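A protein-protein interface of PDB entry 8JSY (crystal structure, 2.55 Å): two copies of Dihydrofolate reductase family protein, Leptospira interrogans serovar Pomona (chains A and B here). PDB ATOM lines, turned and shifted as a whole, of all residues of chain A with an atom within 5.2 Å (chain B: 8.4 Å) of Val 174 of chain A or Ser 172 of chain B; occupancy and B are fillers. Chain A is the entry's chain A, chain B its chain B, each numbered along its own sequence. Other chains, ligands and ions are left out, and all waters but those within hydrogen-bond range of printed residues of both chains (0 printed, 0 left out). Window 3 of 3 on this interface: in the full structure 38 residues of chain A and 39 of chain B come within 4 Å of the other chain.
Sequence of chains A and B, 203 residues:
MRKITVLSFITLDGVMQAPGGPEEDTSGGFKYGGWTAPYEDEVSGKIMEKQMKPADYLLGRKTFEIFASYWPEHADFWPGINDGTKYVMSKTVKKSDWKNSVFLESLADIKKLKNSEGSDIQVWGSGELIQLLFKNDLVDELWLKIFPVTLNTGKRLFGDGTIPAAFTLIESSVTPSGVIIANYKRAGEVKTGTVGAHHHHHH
Of chain B, only Leu 169 (3.3 Å) and Ser 172 (3.1 Å) come within 4 Å of Val 174 of chain A. Ser 172 of chain B touches one residue of chain A. Printed residues of chain A within 4 Å of Val 174 of chain B: Ser 172. Of the printed residues of chain A, Tyr 184 of chain B touches Ile 180. Printed residues of chain B within 4 Å of Ser 172 of chain A: Val 174. Of the printed residues of chain B, Gly 178 of chain A touches Leu 169 (3.9 Å). Ser 173 of chain B touches none of the printed residues of chain A. The nearest residue of chain B that does not touch Val 174 of chain A is Ser 173 of chain B (5.9 Å).
Hydrophobic or aromatic side chains of chain A that line the printed part of chain B: Val 174 and Ile 180. Among the printed residues, 6 pairs touch across the chains. Among the printed residues, no Asp or Glu carboxylate lies within 4 Å of a Lys or Arg side-chain nitrogen of the other chain.
Ser 172 of chain A touches Val 174 of chain B, and with the chains exchanged Val 174 of chain A touches Ser 172 of chain B. 7 positions are printed for both chains.
Ser 172 of chain A touches Val 174 of chain B. Val 174 of chain A touches Leu 169 of chain B. Val 174 of chain A touches Ser 172 of chain B (CG2 to OG, 3.1 Å). CA of Gly 178 of chain A touches CB of Leu 169 of chain B, 3.9 Å away. Leu 169 of chain B touches Ile 180 of chain A (CD1 to CD1, 3.9 Å). Tyr 184 of chain B touches Ile 180 of chain A.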
ATOM      1  N   SER A 172      16.829  11.262  -0.681  1.00  0.00           N
ATOM      2  CA  SER A 172      15.626  11.863  -1.230  1.00  0.00           C
ATOM      3  C   SER A 172      15.846  13.360  -1.362  1.00  0.00           C
ATOM      4  O   SER A 172      16.820  13.916  -0.848  1.00  0.00           O
ATOM      5  CB  SER A 172      14.401  11.577  -0.359  1.00  0.00           C
ATOM      6  OG  SER A 172      13.636  12.757  -0.168  1.00  0.00           O
ATOM      7  N   SER A 173      14.926  14.014  -2.063  1.00  0.00           N
ATOM      8  CA  SER A 173      15.066  15.426  -2.391  1.00  0.00           C
ATOM      9  C   SER A 173      13.748  15.898  -2.964  1.00  0.00           C
ATOM     10  O   SER A 173      12.904  15.094  -3.369  1.00  0.00           O
ATOM     11  CB  SER A 173      16.194  15.689  -3.408  1.00  0.00           C
ATOM     12  OG  SER A 173      17.462  15.242  -2.936  1.00  0.00           O
ATOM     13  N   VAL A 174      13.585  17.215  -2.999  1.00  0.00           N
ATOM     14  CA  VAL A 174      12.423  17.818  -3.628  1.00  0.00           C
ATOM     15  C   VAL A 174      12.916  18.883  -4.594  1.00  0.00           C
ATOM     16  O   VAL A 174      14.016  19.425  -4.460  1.00  0.00           O
ATOM     17  CB  VAL A 174      11.431  18.421  -2.613  1.00  0.00           C
ATOM     18  CG1 VAL A 174      10.077  18.513  -3.225  1.00  0.00           C
ATOM     19  CG2 VAL A 174      11.377  17.598  -1.341  1.00  0.00           C
ATOM     20  N   THR A 175      12.070  19.173  -5.575  1.00  0.00           N
ATOM     21  CA  THR A 175      12.268  20.017  -6.731  1.00  0.00           C
ATOM     22  C   THR A 175      11.328  21.210  -6.677  1.00  0.00           C
ATOM     23  O   THR A 175      10.146  21.051  -6.351  1.00  0.00           O
ATOM     24  CB  THR A 175      12.009  19.205  -8.016  1.00  0.00           C
ATOM     25  OG1 THR A 175      13.214  18.542  -8.409  1.00  0.00           O
ATOM     26  CG2 THR A 175      11.494  20.076  -9.153  1.00  0.00           C
ATOM     27  N   PRO A 176      11.814  22.403  -6.996  1.00  0.00           N
ATOM     28  CA  PRO A 176      10.960  23.600  -6.956  1.00  0.00           C
ATOM     29  C   PRO A 176       9.660  23.452  -7.729  1.00  0.00           C
ATOM     30  O   PRO A 176       8.678  24.147  -7.443  1.00  0.00           O
ATOM     31  CB  PRO A 176      11.857  24.680  -7.572  1.00  0.00           C
ATOM     32  CG  PRO A 176      13.259  24.214  -7.274  1.00  0.00           C
ATOM     33  CD  PRO A 176      13.234  22.719  -7.226  1.00  0.00           C
ATOM     34  N   GLY A 178       8.006  20.570  -7.760  1.00  0.00           N
ATOM     35  CA  GLY A 178       7.229  19.568  -7.064  1.00  0.00           C
ATOM     36  C   GLY A 178       7.505  18.135  -7.459  1.00  0.00           C
ATOM     37  O   GLY A 178       6.589  17.308  -7.419  1.00  0.00           O
ATOM     38  N   VAL A 179       8.728  17.817  -7.851  1.00  0.00           N
ATOM     39  CA  VAL A 179       9.111  16.458  -8.194  1.00  0.00           C
ATOM     40  C   VAL A 179       9.898  15.923  -7.018  1.00  0.00           C
ATOM     41  O   VAL A 179      10.738  16.638  -6.453  1.00  0.00           O
ATOM     42  CB  VAL A 179       9.936  16.407  -9.492  1.00  0.00           C
ATOM     43  CG1 VAL A 179      10.258  14.964  -9.870  1.00  0.00           C
ATOM     44  CG2 VAL A 179       9.178  17.079 -10.618  1.00  0.00           C
ATOM     45  N   ILE A 180       9.597  14.689  -6.615  1.00  0.00           N
ATOM     46  CA  ILE A 180      10.333  14.036  -5.539  1.00  0.00           C
ATOM     47  C   ILE A 180      11.394  13.143  -6.158  1.00  0.00           C
ATOM     48  O   ILE A 180      11.094  12.309  -7.025  1.00  0.00           O
ATOM     49  CB  ILE A 180       9.407  13.225  -4.614  1.00  0.00           C
ATOM     50  CG1 ILE A 180       8.511  14.149  -3.799  1.00  0.00           C
ATOM     51  CG2 ILE A 180      10.223  12.368  -3.671  1.00  0.00           C
ATOM     52  CD1 ILE A 180       7.244  14.491  -4.510  1.00  0.00           C
ATOM     53  N   ILE A 181      12.632  13.324  -5.727  1.00  0.00           N
ATOM     54  CA  ILE A 181      13.713  12.412  -6.068  1.00  0.00           C
ATOM     55  C   ILE A 181      13.802  11.388  -4.947  1.00  0.00           C
ATOM     56  O   ILE A 181      13.825  11.760  -3.769  1.00  0.00           O
ATOM     57  CB  ILE A 181      15.043  13.170  -6.238  1.00  0.00           C
ATOM     58  CG1 ILE A 181      14.842  14.420  -7.093  1.00  0.00           C
ATOM     59  CG2 ILE A 181      16.115  12.264  -6.828  1.00  0.00           C
ATOM     60  CD1 ILE A 181      14.509  14.129  -8.519  1.00  0.00           C
ATOM     61  N   LEU B 144      -0.175  11.514   1.353  1.00  0.00           N
ATOM     62  CA  LEU B 144       0.318  10.175   1.119  1.00  0.00           C
ATOM     63  C   LEU B 144       1.550   9.910   1.963  1.00  0.00           C
ATOM     64  O   LEU B 144       2.381  10.800   2.181  1.00  0.00           O
ATOM     65  CB  LEU B 144       0.658   9.988  -0.359  1.00  0.00           C
ATOM     66  CG  LEU B 144      -0.321  10.621  -1.351  1.00  0.00           C
ATOM     67  CD1 LEU B 144       0.104  10.315  -2.773  1.00  0.00           C
ATOM     68  CD2 LEU B 144      -1.763  10.145  -1.118  1.00  0.00           C
ATOM     69  N   ILE B 146       4.461   7.165   1.531  1.00  0.00           N
ATOM     70  CA  ILE B 146       4.996   6.201   0.577  1.00  0.00           C
ATOM     71  C   ILE B 146       6.059   5.374   1.272  1.00  0.00           C
ATOM     72  O   ILE B 146       7.020   5.923   1.833  1.00  0.00           O
ATOM     73  CB  ILE B 146       5.563   6.908  -0.658  1.00  0.00           C
ATOM     74  CG1 ILE B 146       4.471   7.795  -1.259  1.00  0.00           C
ATOM     75  CG2 ILE B 146       6.088   5.877  -1.657  1.00  0.00           C
ATOM     76  CD1 ILE B 146       4.970   8.888  -2.150  1.00  0.00           C
ATOM     77  N   LEU B 169       2.633  19.968  -5.313  1.00  0.00           N
ATOM     78  CA  LEU B 169       3.220  19.426  -4.092  1.00  0.00           C
ATOM     79  C   LEU B 169       3.258  20.532  -3.056  1.00  0.00           C
ATOM     80  O   LEU B 169       4.109  21.426  -3.119  1.00  0.00           O
ATOM     81  CB  LEU B 169       4.621  18.863  -4.319  1.00  0.00           C
ATOM     82  CG  LEU B 169       5.325  18.517  -2.993  1.00  0.00           C
ATOM     83  CD1 LEU B 169       5.069  17.104  -2.506  1.00  0.00           C
ATOM     84  CD2 LEU B 169       6.794  18.749  -3.068  1.00  0.00           C
ATOM     85  N   ILE B 170       2.349  20.463  -2.078  1.00  0.00           N
ATOM     86  CA  ILE B 170       2.307  21.499  -1.053  1.00  0.00           C
ATOM     87  C   ILE B 170       3.190  21.172   0.152  1.00  0.00           C
ATOM     88  O   ILE B 170       3.561  22.093   0.890  1.00  0.00           O
ATOM     89  CB  ILE B 170       0.842  21.842  -0.681  1.00  0.00           C
ATOM     90  CG1 ILE B 170      -0.013  20.661  -0.203  1.00  0.00           C
ATOM     91  CG2 ILE B 170       0.128  22.514  -1.849  1.00  0.00           C
ATOM     92  CD1 ILE B 170       0.361  20.122   1.157  1.00  0.00           C
ATOM     93  N   GLU B 171       3.552  19.909   0.373  1.00  0.00           N
ATOM     94  CA  GLU B 171       4.585  19.668   1.378  1.00  0.00           C
ATOM     95  C   GLU B 171       5.147  18.266   1.216  1.00  0.00           C
ATOM     96  O   GLU B 171       4.527  17.402   0.594  1.00  0.00           O
ATOM     97  CB  GLU B 171       4.057  19.856   2.804  1.00  0.00           C
ATOM     98  CG  GLU B 171       5.158  20.211   3.805  1.00  0.00           C
ATOM     99  CD  GLU B 171       4.991  19.542   5.169  1.00  0.00           C
ATOM    100  OE1 GLU B 171       5.990  19.511   5.936  1.00  0.00           O
ATOM    101  OE2 GLU B 171       3.865  19.067   5.475  1.00  0.00           O
ATOM    102  N   SER B 172       6.318  18.039   1.818  1.00  0.00           N
ATOM    103  CA  SER B 172       6.949  16.726   1.772  1.00  0.00           C
ATOM    104  C   SER B 172       8.097  16.682   2.764  1.00  0.00           C
ATOM    105  O   SER B 172       8.719  17.706   3.057  1.00  0.00           O
ATOM    106  CB  SER B 172       7.484  16.391   0.376  1.00  0.00           C
ATOM    107  OG  SER B 172       8.848  16.764   0.277  1.00  0.00           O
ATOM    108  N   SER B 173       8.390  15.471   3.237  1.00  0.00           N
ATOM    109  CA  SER B 173       9.481  15.222   4.176  1.00  0.00           C
ATOM    110  C   SER B 173       9.747  13.722   4.215  1.00  0.00           C
ATOM    111  O   SER B 173       9.044  12.940   3.578  1.00  0.00           O
ATOM    112  CB  SER B 173       9.147  15.761   5.566  1.00  0.00           C
ATOM    113  OG  SER B 173       8.655  14.720   6.389  1.00  0.00           O
ATOM    114  N   VAL B 174      10.783  13.324   4.959  1.00  0.00           N
ATOM    115  CA  VAL B 174      11.145  11.916   5.101  1.00  0.00           C
ATOM    116  C   VAL B 174      11.301  11.564   6.574  1.00  0.00           C
ATOM    117  O   VAL B 174      11.792  12.369   7.373  1.00  0.00           O
ATOM    118  CB  VAL B 174      12.437  11.546   4.334  1.00  0.00           C
ATOM    119  CG1 VAL B 174      12.362  12.011   2.881  1.00  0.00           C
ATOM    120  CG2 VAL B 174      13.685  12.088   5.036  1.00  0.00           C
ATOM    121  N   THR B 175      10.860  10.340   6.937  1.00  0.00           N
ATOM    122  CA  THR B 175      11.021   9.761   8.259  1.00  0.00           C
ATOM    123  C   THR B 175      12.349   9.021   8.362  1.00  0.00           C
ATOM    124  O   THR B 175      12.885   8.544   7.354  1.00  0.00           O
ATOM    125  CB  THR B 175       9.888   8.782   8.571  1.00  0.00           C
ATOM    126  OG1 THR B 175      10.135   7.528   7.916  1.00  0.00           O
ATOM    127  CG2 THR B 175       8.566   9.327   8.123  1.00  0.00           C
ATOM    128  N   VAL B 179      10.157   6.590   5.126  1.00  0.00           N
ATOM    129  CA  VAL B 179       8.868   6.808   4.494  1.00  0.00           C
ATOM    130  C   VAL B 179       8.834   8.243   3.990  1.00  0.00           C
ATOM    131  O   VAL B 179       9.451   9.146   4.569  1.00  0.00           O
ATOM    132  CB  VAL B 179       7.733   6.500   5.495  1.00  0.00           C
ATOM    133  CG1 VAL B 179       6.346   6.864   4.941  1.00  0.00           C
ATOM    134  CG2 VAL B 179       7.802   5.042   5.910  1.00  0.00           C
ATOM    135  N   ILE B 180       8.136   8.466   2.885  1.00  0.00           N
ATOM    136  CA  ILE B 180       8.074   9.793   2.289  1.00  0.00           C
ATOM    137  C   ILE B 180       6.682  10.361   2.511  1.00  0.00           C
ATOM    138  O   ILE B 180       5.676   9.760   2.105  1.00  0.00           O
ATOM    139  CB  ILE B 180       8.455   9.764   0.802  1.00  0.00           C
ATOM    140  CG1 ILE B 180       9.932   9.395   0.668  1.00  0.00           C
ATOM    141  CG2 ILE B 180       8.173  11.107   0.131  1.00  0.00           C
ATOM    142  CD1 ILE B 180      10.272   8.841  -0.643  1.00  0.00           C
ATOM    143  N   ILE B 181       6.622  11.499   3.181  1.00  0.00           N
ATOM    144  CA  ILE B 181       5.365  12.193   3.396  1.00  0.00           C
ATOM    145  C   ILE B 181       5.219  13.204   2.275  1.00  0.00           C
ATOM    146  O   ILE B 181       6.048  14.109   2.132  1.00  0.00           O
ATOM    147  CB  ILE B 181       5.307  12.881   4.771  1.00  0.00           C
ATOM    148  CG1 ILE B 181       5.361  11.860   5.913  1.00  0.00           C
ATOM    149  CG2 ILE B 181       4.045  13.731   4.875  1.00  0.00           C
ATOM    150  CD1 ILE B 181       6.745  11.430   6.272  1.00  0.00           C
ATOM    151  N   ALA B 182       4.172  13.047   1.484  1.00  0.00           N
ATOM    152  CA  ALA B 182       3.931  13.899   0.333  1.00  0.00           C
ATOM    153  C   ALA B 182       2.478  14.323   0.395  1.00  0.00           C
ATOM    154  O   ALA B 182       1.578  13.498   0.222  1.00  0.00           O
ATOM    155  CB  ALA B 182       4.236  13.163  -0.971  1.00  0.00           C
ATOM    156  N   ASN B 183       2.243  15.592   0.676  1.00  0.00           N
ATOM    157  CA  ASN B 183       0.900  16.137   0.646  1.00  0.00           C
ATOM    158  C   ASN B 183       0.818  17.011  -0.595  1.00  0.00           C
ATOM    159  O   ASN B 183       1.705  17.843  -0.832  1.00  0.00           O
ATOM    160  CB  ASN B 183       0.562  16.918   1.928  1.00  0.00           C
ATOM    161  CG  ASN B 183       0.950  16.172   3.235  1.00  0.00           C
ATOM    162  OD1 ASN B 183       1.264  14.969   3.232  1.00  0.00           O
ATOM    163  ND2 ASN B 183       0.919  16.899   4.356  1.00  0.00           N
ATOM    164  N   TYR B 184      -0.248  16.801  -1.370  1.00  0.00           N
ATOM    165  CA  TYR B 184      -0.485  17.357  -2.690  1.00  0.00           C
ATOM    166  C   TYR B 184      -1.814  18.078  -2.700  1.00  0.00           C
ATOM    167  O   TYR B 184      -2.745  17.700  -1.983  1.00  0.00           O
ATOM    168  CB  TYR B 184      -0.553  16.255  -3.770  1.00  0.00           C
ATOM    169  CG  TYR B 184       0.773  15.606  -4.082  1.00  0.00           C
ATOM    170  CD1 TYR B 184       1.867  16.357  -4.483  1.00  0.00           C
ATOM    171  CD2 TYR B 184       0.950  14.242  -3.902  1.00  0.00           C
ATOM    172  CE1 TYR B 184       3.084  15.753  -4.749  1.00  0.00           C
ATOM    173  CE2 TYR B 184       2.156  13.639  -4.154  1.00  0.00           C
ATOM    174  CZ  TYR B 184       3.218  14.401  -4.575  1.00  0.00           C
ATOM    175  OH  TYR B 184       4.417  13.788  -4.820  1.00  0.00           O
